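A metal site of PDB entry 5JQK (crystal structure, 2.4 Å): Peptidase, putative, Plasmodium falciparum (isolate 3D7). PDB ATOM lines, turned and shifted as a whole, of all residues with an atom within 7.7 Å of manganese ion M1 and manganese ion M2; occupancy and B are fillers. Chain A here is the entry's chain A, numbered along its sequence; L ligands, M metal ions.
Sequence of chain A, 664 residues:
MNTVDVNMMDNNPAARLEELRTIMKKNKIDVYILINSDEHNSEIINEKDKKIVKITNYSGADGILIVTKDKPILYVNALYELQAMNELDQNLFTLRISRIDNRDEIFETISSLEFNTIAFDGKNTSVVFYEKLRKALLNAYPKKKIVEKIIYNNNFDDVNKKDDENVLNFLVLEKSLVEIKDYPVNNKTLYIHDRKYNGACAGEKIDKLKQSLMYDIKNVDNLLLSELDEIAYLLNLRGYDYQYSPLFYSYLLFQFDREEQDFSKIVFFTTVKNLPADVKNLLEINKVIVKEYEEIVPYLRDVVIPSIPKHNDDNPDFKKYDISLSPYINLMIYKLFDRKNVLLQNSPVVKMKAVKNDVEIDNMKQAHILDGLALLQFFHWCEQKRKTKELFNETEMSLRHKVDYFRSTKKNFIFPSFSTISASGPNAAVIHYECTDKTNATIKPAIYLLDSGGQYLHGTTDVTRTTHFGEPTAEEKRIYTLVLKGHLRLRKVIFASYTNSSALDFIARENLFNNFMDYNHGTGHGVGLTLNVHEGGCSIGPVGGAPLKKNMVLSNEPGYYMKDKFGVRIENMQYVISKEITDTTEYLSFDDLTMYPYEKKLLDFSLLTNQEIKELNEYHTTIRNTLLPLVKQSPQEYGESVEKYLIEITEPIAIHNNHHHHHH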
ATOM      1  N   SER A 417       2.792  -6.768  19.612  1.00  0.00           N
ATOM      2  CA  SER A 417       3.180  -6.953  18.225  1.00  0.00           C
ATOM      3  C   SER A 417       2.508  -5.941  17.298  1.00  0.00           C
ATOM      4  O   SER A 417       2.888  -5.799  16.135  1.00  0.00           O
ATOM      5  CB  SER A 417       2.847  -8.379  17.770  1.00  0.00           C
ATOM      6  OG  SER A 417       1.479  -8.665  17.958  1.00  0.00           O
ATOM      7  N   PHE A 418       1.499  -5.244  17.825  1.00  0.00           N
ATOM      8  CA  PHE A 418       0.882  -4.119  17.122  1.00  0.00           C
ATOM      9  C   PHE A 418       0.027  -3.333  18.103  1.00  0.00           C
ATOM     10  O   PHE A 418      -0.126  -3.742  19.257  1.00  0.00           O
ATOM     11  CB  PHE A 418       0.044  -4.580  15.925  1.00  0.00           C
ATOM     12  CG  PHE A 418      -1.005  -5.594  16.272  1.00  0.00           C
ATOM     13  CD1 PHE A 418      -2.312  -5.202  16.526  1.00  0.00           C
ATOM     14  CD2 PHE A 418      -0.706  -6.942  16.329  1.00  0.00           C
ATOM     15  CE1 PHE A 418      -3.281  -6.131  16.832  1.00  0.00           C
ATOM     16  CE2 PHE A 418      -1.665  -7.881  16.640  1.00  0.00           C
ATOM     17  CZ  PHE A 418      -2.968  -7.477  16.888  1.00  0.00           C
ATOM     18  N   ILE A 421      -6.321  -3.279  19.284  1.00  0.00           N
ATOM     19  CA  ILE A 421      -7.614  -2.733  18.926  1.00  0.00           C
ATOM     20  C   ILE A 421      -8.631  -3.144  19.980  1.00  0.00           C
ATOM     21  O   ILE A 421      -8.958  -4.324  20.135  1.00  0.00           O
ATOM     22  CB  ILE A 421      -8.091  -3.203  17.551  1.00  0.00           C
ATOM     23  CG1 ILE A 421      -7.058  -2.838  16.482  1.00  0.00           C
ATOM     24  CG2 ILE A 421      -9.439  -2.599  17.217  1.00  0.00           C
ATOM     25  CD1 ILE A 421      -7.370  -3.422  15.125  1.00  0.00           C
ATOM     26  N   LEU A 450     -11.698  -7.390  20.567  1.00  0.00           N
ATOM     27  CA  LEU A 450     -10.311  -7.202  20.991  1.00  0.00           C
ATOM     28  C   LEU A 450      -9.350  -7.877  20.022  1.00  0.00           C
ATOM     29  O   LEU A 450      -9.279  -9.110  19.972  1.00  0.00           O
ATOM     30  CB  LEU A 450     -10.110  -7.757  22.407  1.00  0.00           C
ATOM     31  CG  LEU A 450      -8.708  -7.624  22.992  1.00  0.00           C
ATOM     32  CD1 LEU A 450      -8.436  -6.193  23.415  1.00  0.00           C
ATOM     33  CD2 LEU A 450      -8.491  -8.580  24.158  1.00  0.00           C
ATOM     34  N   ASP A 451      -8.582  -7.077  19.296  1.00  0.00           N
ATOM     35  CA  ASP A 451      -7.532  -7.603  18.417  1.00  0.00           C
ATOM     36  C   ASP A 451      -6.194  -7.213  19.024  1.00  0.00           C
ATOM     37  O   ASP A 451      -5.876  -6.037  19.160  1.00  0.00           O
ATOM     38  CB  ASP A 451      -7.658  -7.062  16.993  1.00  0.00           C
ATOM     39  CG  ASP A 451      -6.807  -7.839  15.994  1.00  0.00           C
ATOM     40  OD1 ASP A 451      -5.953  -8.641  16.419  1.00  0.00           O
ATOM     41  OD2 ASP A 451      -6.986  -7.652  14.769  1.00  0.00           O
ATOM     42  N   SER A 452      -5.419  -8.225  19.406  1.00  0.00           N
ATOM     43  CA  SER A 452      -4.158  -7.985  20.090  1.00  0.00           C
ATOM     44  C   SER A 452      -3.179  -9.111  19.856  1.00  0.00           C
ATOM     45  O   SER A 452      -3.546 -10.199  19.389  1.00  0.00           O
ATOM     46  CB  SER A 452      -4.387  -7.800  21.584  1.00  0.00           C
ATOM     47  OG  SER A 452      -4.966  -8.969  22.158  1.00  0.00           O
ATOM     48  N   GLY A 453      -1.914  -8.840  20.149  1.00  0.00           N
ATOM     49  CA  GLY A 453      -0.873  -9.828  20.015  1.00  0.00           C
ATOM     50  C   GLY A 453       0.372  -9.320  20.705  1.00  0.00           C
ATOM     51  O   GLY A 453       0.404  -8.191  21.204  1.00  0.00           O
ATOM     52  N   THR A 461       2.516 -13.227  17.915  1.00  0.00           N
ATOM     53  CA  THR A 461       1.132 -13.663  18.011  1.00  0.00           C
ATOM     54  C   THR A 461       0.159 -12.603  17.540  1.00  0.00           C
ATOM     55  O   THR A 461       0.394 -11.409  17.688  1.00  0.00           O
ATOM     56  CB  THR A 461       0.770 -14.033  19.455  1.00  0.00           C
ATOM     57  OG1 THR A 461       0.807 -12.866  20.274  1.00  0.00           O
ATOM     58  CG2 THR A 461       1.743 -15.069  20.005  1.00  0.00           C
ATOM     59  N   ASP A 462      -0.933 -13.057  16.928  1.00  0.00           N
ATOM     60  CA  ASP A 462      -2.021 -12.185  16.499  1.00  0.00           C
ATOM     61  C   ASP A 462      -3.354 -12.904  16.743  1.00  0.00           C
ATOM     62  O   ASP A 462      -3.585 -13.973  16.195  1.00  0.00           O
ATOM     63  CB  ASP A 462      -1.836 -11.814  15.018  1.00  0.00           C
ATOM     64  CG  ASP A 462      -2.868 -10.828  14.511  1.00  0.00           C
ATOM     65  OD1 ASP A 462      -2.854 -10.556  13.304  1.00  0.00           O
ATOM     66  OD2 ASP A 462      -3.699 -10.329  15.306  1.00  0.00           O
ATOM     67  N   VAL A 463      -4.224 -12.321  17.563  1.00  0.00           N
ATOM     68  CA  VAL A 463      -5.485 -12.981  17.891  1.00  0.00           C
ATOM     69  C   VAL A 463      -6.625 -11.986  18.100  1.00  0.00           C
ATOM     70  O   VAL A 463      -6.429 -10.939  18.712  1.00  0.00           O
ATOM     71  CB  VAL A 463      -5.336 -13.862  19.171  1.00  0.00           C
ATOM     72  CG1 VAL A 463      -4.660 -13.090  20.297  1.00  0.00           C
ATOM     73  CG2 VAL A 463      -6.683 -14.426  19.627  1.00  0.00           C
ATOM     74  N   THR A 464      -7.803 -12.319  17.583  1.00  0.00           N
ATOM     75  CA  THR A 464      -8.993 -11.509  17.837  1.00  0.00           C
ATOM     76  C   THR A 464     -10.101 -12.353  18.443  1.00  0.00           C
ATOM     77  O   THR A 464     -10.390 -13.459  17.976  1.00  0.00           O
ATOM     78  CB  THR A 464      -9.538 -10.841  16.556  1.00  0.00           C
ATOM     79  OG1 THR A 464      -8.476 -10.210  15.845  1.00  0.00           O
ATOM     80  CG2 THR A 464     -10.616  -9.823  16.901  1.00  0.00           C
ATOM     81  N   ARG A 465     -10.727 -11.822  19.487  1.00  0.00           N
ATOM     82  CA  ARG A 465     -11.920 -12.430  20.041  1.00  0.00           C
ATOM     83  C   ARG A 465     -12.998 -11.374  20.169  1.00  0.00           C
ATOM     84  O   ARG A 465     -12.708 -10.222  20.466  1.00  0.00           O
ATOM     85  CB  ARG A 465     -11.634 -13.089  21.393  1.00  0.00           C
ATOM     86  CG  ARG A 465     -10.842 -14.374  21.306  1.00  0.00           C
ATOM     87  CD  ARG A 465     -11.585 -15.383  20.448  1.00  0.00           C
ATOM     88  NE  ARG A 465     -10.930 -16.692  20.418  1.00  0.00           N
ATOM     89  CZ  ARG A 465     -10.130 -17.105  19.445  1.00  0.00           C
ATOM     90  NH1 ARG A 465      -9.858 -16.313  18.419  1.00  0.00           N
ATOM     91  NH2 ARG A 465      -9.593 -18.315  19.493  1.00  0.00           N
ATOM     92  N   GLY A 522      -8.683  -8.825   4.030  1.00  0.00           N
ATOM     93  CA  GLY A 522      -8.300 -10.178   3.668  1.00  0.00           C
ATOM     94  C   GLY A 522      -8.650 -11.141   4.793  1.00  0.00           C
ATOM     95  O   GLY A 522      -8.912 -10.722   5.912  1.00  0.00           O
ATOM     96  N   THR A 523      -8.685 -12.434   4.474  1.00  0.00           N
ATOM     97  CA  THR A 523      -9.044 -13.424   5.476  1.00  0.00           C
ATOM     98  C   THR A 523      -7.846 -13.786   6.354  1.00  0.00           C
ATOM     99  O   THR A 523      -8.003 -14.039   7.549  1.00  0.00           O
ATOM    100  CB  THR A 523      -9.598 -14.699   4.829  1.00  0.00           C
ATOM    101  OG1 THR A 523     -10.773 -14.372   4.076  1.00  0.00           O
ATOM    102  CG2 THR A 523      -9.968 -15.717   5.898  1.00  0.00           C
ATOM    103  N   GLY A 524      -6.657 -13.784   5.770  1.00  0.00           N
ATOM    104  CA  GLY A 524      -5.464 -14.092   6.539  1.00  0.00           C
ATOM    105  C   GLY A 524      -4.179 -13.543   5.964  1.00  0.00           C
ATOM    106  O   GLY A 524      -4.044 -13.358   4.751  1.00  0.00           O
ATOM    107  N   HIS A 525      -3.225 -13.302   6.846  1.00  0.00           N
ATOM    108  CA  HIS A 525      -1.909 -12.806   6.464  1.00  0.00           C
ATOM    109  C   HIS A 525      -0.852 -13.721   7.046  1.00  0.00           C
ATOM    110  O   HIS A 525      -1.100 -14.397   8.056  1.00  0.00           O
ATOM    111  CB  HIS A 525      -1.698 -11.371   6.966  1.00  0.00           C
ATOM    112  CG  HIS A 525      -1.939 -11.206   8.432  1.00  0.00           C
ATOM    113  ND1 HIS A 525      -1.025 -11.605   9.385  1.00  0.00           N
ATOM    114  CD2 HIS A 525      -2.988 -10.675   9.111  1.00  0.00           C
ATOM    115  CE1 HIS A 525      -1.501 -11.344  10.589  1.00  0.00           C
ATOM    116  NE2 HIS A 525      -2.697 -10.777  10.448  1.00  0.00           N
ATOM    117  N   GLY A 526       0.319 -13.746   6.430  1.00  0.00           N
ATOM    118  CA  GLY A 526       1.438 -14.493   6.992  1.00  0.00           C
ATOM    119  C   GLY A 526       1.910 -13.781   8.237  1.00  0.00           C
ATOM    120  O   GLY A 526       1.655 -12.597   8.408  1.00  0.00           O
ATOM    121  N   VAL A 527       2.576 -14.518   9.128  1.00  0.00           N
ATOM    122  CA  VAL A 527       3.096 -13.928  10.362  1.00  0.00           C
ATOM    123  C   VAL A 527       4.541 -14.346  10.588  1.00  0.00           C
ATOM    124  O   VAL A 527       4.875 -15.524  10.530  1.00  0.00           O
ATOM    125  CB  VAL A 527       2.248 -14.327  11.584  1.00  0.00           C
ATOM    126  CG1 VAL A 527       2.788 -13.657  12.842  1.00  0.00           C
ATOM    127  CG2 VAL A 527       0.789 -13.942  11.368  1.00  0.00           C
ATOM    128  N   VAL A 533       4.089  -8.703  12.459  1.00  0.00           N
ATOM    129  CA  VAL A 533       2.819  -9.373  12.615  1.00  0.00           C
ATOM    130  C   VAL A 533       2.160  -9.542  11.246  1.00  0.00           C
ATOM    131  O   VAL A 533       1.328 -10.422  11.048  1.00  0.00           O
ATOM    132  CB  VAL A 533       1.908  -8.595  13.590  1.00  0.00           C
ATOM    133  CG1 VAL A 533       1.471  -7.275  12.983  1.00  0.00           C
ATOM    134  CG2 VAL A 533       0.715  -9.436  14.000  1.00  0.00           C
ATOM    135  N   HIS A 534       2.539  -8.697  10.284  1.00  0.00           N
ATOM    136  CA  HIS A 534       2.126  -8.872   8.892  1.00  0.00           C
ATOM    137  C   HIS A 534       3.323  -9.212   8.020  1.00  0.00           C
ATOM    138  O   HIS A 534       4.168  -8.368   7.740  1.00  0.00           O
ATOM    139  CB  HIS A 534       1.445  -7.608   8.367  1.00  0.00           C
ATOM    140  CG  HIS A 534       0.161  -7.285   9.066  1.00  0.00           C
ATOM    141  ND1 HIS A 534      -0.331  -6.006   9.167  1.00  0.00           N
ATOM    142  CD2 HIS A 534      -0.736  -8.087   9.701  1.00  0.00           C
ATOM    143  CE1 HIS A 534      -1.475  -6.020   9.838  1.00  0.00           C
ATOM    144  NE2 HIS A 534      -1.739  -7.272  10.172  1.00  0.00           N
ATOM    145  N   LEU A 554      -0.238 -18.771   9.096  1.00  0.00           N
ATOM    146  CA  LEU A 554      -1.193 -17.790   8.629  1.00  0.00           C
ATOM    147  C   LEU A 554      -2.256 -17.453   9.667  1.00  0.00           C
ATOM    148  O   LEU A 554      -2.566 -18.278  10.537  1.00  0.00           O
ATOM    149  CB  LEU A 554      -1.883 -18.290   7.343  1.00  0.00           C
ATOM    150  CG  LEU A 554      -0.951 -18.449   6.143  1.00  0.00           C
ATOM    151  CD1 LEU A 554      -1.131 -19.804   5.494  1.00  0.00           C
ATOM    152  CD2 LEU A 554      -1.172 -17.331   5.145  1.00  0.00           C
ATOM    153  N   SER A 555      -2.785 -16.251   9.591  1.00  0.00           N
ATOM    154  CA  SER A 555      -3.948 -15.893  10.376  1.00  0.00           C
ATOM    155  C   SER A 555      -5.219 -16.402   9.712  1.00  0.00           C
ATOM    156  O   SER A 555      -5.255 -16.622   8.503  1.00  0.00           O
ATOM    157  CB  SER A 555      -4.014 -14.374  10.595  1.00  0.00           C
ATOM    158  OG  SER A 555      -4.282 -13.689   9.387  1.00  0.00           O
ATOM    159  N   ASN A 556      -6.251 -16.622  10.513  1.00  0.00           N
ATOM    160  CA  ASN A 556      -7.565 -16.933   9.995  1.00  0.00           C
ATOM    161  C   ASN A 556      -8.535 -15.974  10.686  1.00  0.00           C
ATOM    162  O   ASN A 556      -8.866 -16.177  11.845  1.00  0.00           O
ATOM    163  CB  ASN A 556      -7.891 -18.405  10.280  1.00  0.00           C
ATOM    164  CG  ASN A 556      -9.368 -18.755  10.142  1.00  0.00           C
ATOM    165  OD1 ASN A 556     -10.159 -18.027   9.537  1.00  0.00           O
ATOM    166  ND2 ASN A 556      -9.746 -19.881  10.724  1.00  0.00           N
ATOM    167  N   GLU A 557      -9.018 -14.969   9.970  1.00  0.00           N
ATOM    168  CA  GLU A 557      -9.788 -13.910  10.619  1.00  0.00           C
ATOM    169  C   GLU A 557     -10.912 -13.312   9.796  1.00  0.00           C
ATOM    170  O   GLU A 557     -10.859 -12.139   9.427  1.00  0.00           O
ATOM    171  CB  GLU A 557      -8.862 -12.764  11.073  1.00  0.00           C
ATOM    172  CG  GLU A 557      -7.808 -12.311  10.077  1.00  0.00           C
ATOM    173  CD  GLU A 557      -6.921 -11.216  10.649  1.00  0.00           C
ATOM    174  OE1 GLU A 557      -7.429 -10.381  11.425  1.00  0.00           O
ATOM    175  OE2 GLU A 557      -5.707 -11.184  10.333  1.00  0.00           O
ATOM    176  N   ARG A 569     -15.093  -9.800  14.664  1.00  0.00           N
ATOM    177  CA  ARG A 569     -14.000 -10.519  14.022  1.00  0.00           C
ATOM    178  C   ARG A 569     -13.527 -11.655  14.913  1.00  0.00           C
ATOM    179  O   ARG A 569     -13.447 -11.500  16.139  1.00  0.00           O
ATOM    180  CB  ARG A 569     -12.829  -9.591  13.669  1.00  0.00           C
ATOM    181  CG  ARG A 569     -11.678 -10.293  12.969  1.00  0.00           C
ATOM    182  CD  ARG A 569     -10.705  -9.325  12.289  1.00  0.00           C
ATOM    183  NE  ARG A 569     -10.013  -8.451  13.237  1.00  0.00           N
ATOM    184  CZ  ARG A 569     -10.317  -7.173  13.427  1.00  0.00           C
ATOM    185  NH1 ARG A 569     -11.306  -6.619  12.740  1.00  0.00           N
ATOM    186  NH2 ARG A 569      -9.632  -6.450  14.305  1.00  0.00           N
ATOM    187  N   GLU A 571     -10.347 -14.307  15.121  1.00  0.00           N
ATOM    188  CA  GLU A 571      -9.030 -14.551  14.532  1.00  0.00           C
ATOM    189  C   GLU A 571      -8.184 -15.582  15.263  1.00  0.00           C
ATOM    190  O   GLU A 571      -7.993 -15.504  16.478  1.00  0.00           O
ATOM    191  CB  GLU A 571      -8.241 -13.240  14.439  1.00  0.00           C
ATOM    192  CG  GLU A 571      -6.814 -13.407  13.913  1.00  0.00           C
ATOM    193  CD  GLU A 571      -6.071 -12.089  13.820  1.00  0.00           C
ATOM    194  OE1 GLU A 571      -6.427 -11.138  14.536  1.00  0.00           O
ATOM    195  OE2 GLU A 571      -5.124 -12.010  13.011  1.00  0.00           O
ATOM    196  N   ASN A 572      -7.690 -16.543  14.507  1.00  0.00           N
ATOM    197  CA  ASN A 572      -6.698 -17.490  14.985  1.00  0.00           C
ATOM    198  C   ASN A 572      -5.448 -17.421  14.120  1.00  0.00           C
ATOM    199  O   ASN A 572      -5.490 -16.908  13.003  1.00  0.00           O
ATOM    200  CB  ASN A 572      -7.229 -18.912  14.969  1.00  0.00           C
ATOM    201  CG  ASN A 572      -8.041 -19.249  16.192  1.00  0.00           C
ATOM    202  OD1 ASN A 572      -8.461 -18.363  16.933  1.00  0.00           O
ATOM    203  ND2 ASN A 572      -8.267 -20.539  16.412  1.00  0.00           N
ATOM    204  N   MET A 573      -4.345 -17.913  14.648  1.00  0.00           N
ATOM    205  CA  MET A 573      -3.189 -18.222  13.810  1.00  0.00           C
ATOM    206  C   MET A 573      -3.094 -19.738  13.709  1.00  0.00           C
ATOM    207  O   MET A 573      -3.417 -20.453  14.657  1.00  0.00           O
ATOM    208  CB  MET A 573      -1.911 -17.614  14.363  1.00  0.00           C
ATOM    209  CG  MET A 573      -1.652 -16.173  13.940  1.00  0.00           C
ATOM    210  SD  MET A 573      -0.348 -15.418  14.940  1.00  0.00           S
ATOM    211  CE  MET A 573       1.061 -16.356  14.374  1.00  0.00           C
HETATM  212  P1  LIG L   1      -4.290  -7.426  12.419  1.00  0.00           P
HETATM  213  O1  LIG L   1      -2.964  -7.301  13.148  1.00  0.00           O
HETATM  214  O2  LIG L   1      -4.953  -8.739  12.770  1.00  0.00           O
HETATM  215  O3  LIG L   1      -4.056  -7.374  10.936  1.00  0.00           O
HETATM  216  O4  LIG L   1      -5.190  -6.278  12.829  1.00  0.00           O
HETATM  217 MN    MN M   1      -4.248 -10.525  11.944  1.00  0.00          MN
HETATM  218 MN    MN M   2      -5.274  -9.397  14.731  1.00  0.00          MN
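The backbone NH of Asp 462 is in hydrogen-bond range of the side-chain sulfur of Met 573.
The backbone carbonyl oxygen (O) of Asp 451 sits at hydrogen-bond distance from the backbone NH (N) of Ile 421 (2.8 Å).
The backbone NH (N) of Glu 571 sits at hydrogen-bond distance from the backbone carbonyl oxygen (O) of Thr 464 (3.0 Å).
The guanidinium group of Arg 465 lies within hydrogen-bond range of the backbone carbonyl oxygen of Glu 571 (2.8 Å).
N of His 525 is in hydrogen-bond range of OG of Ser 555 (2.8 Å).
ND1 of His 525 lies close to O of Val 533, 3.1 Å away.
The side-chain hydroxyl (OG) of Ser 555 lies close to the side-chain carboxylate (OE2) of Glu 557, 3.0 Å away.
The side-chain carboxylate of Glu 557 is in salt-bridge range of the guanidinium group of Arg 569.
Along chain A the residues within 4 Å of manganese ion M1 span positions 462 to 571.
The nearest printed residue that does not touch manganese ion M1 is Ser 555 (4.1 Å).
Phe 418 touches manganese ion M2.
Thr 464 touches manganese ion M2 (OG1 to MN, 3.5 Å).
Manganese ion M1 is bound by OD1 of Asp 462, at 1.9 Å.
OE2 of Glu 571 binds manganese ion M1 (2.0 Å).
O2 of the ligand binds manganese ion M1, 2.1 Å away.
Manganese ion M1 is bound by a ring nitrogen (NE2) of His 525.
Manganese ion M1 is bound by OE2 of Glu 557 (2.3 Å).
OD2 of Asp 462 is bound to manganese ion M2 (1.9 Å).
Manganese ion M2 is bound by OD1 of Asp 451 (2.0 Å).
Manganese ion M2 is bound by O2 of the ligand (2.1 Å).
OE1 of Glu 571 is bound to manganese ion M2.
OD2 of Asp 451 binds manganese ion M2 (2.4 Å).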
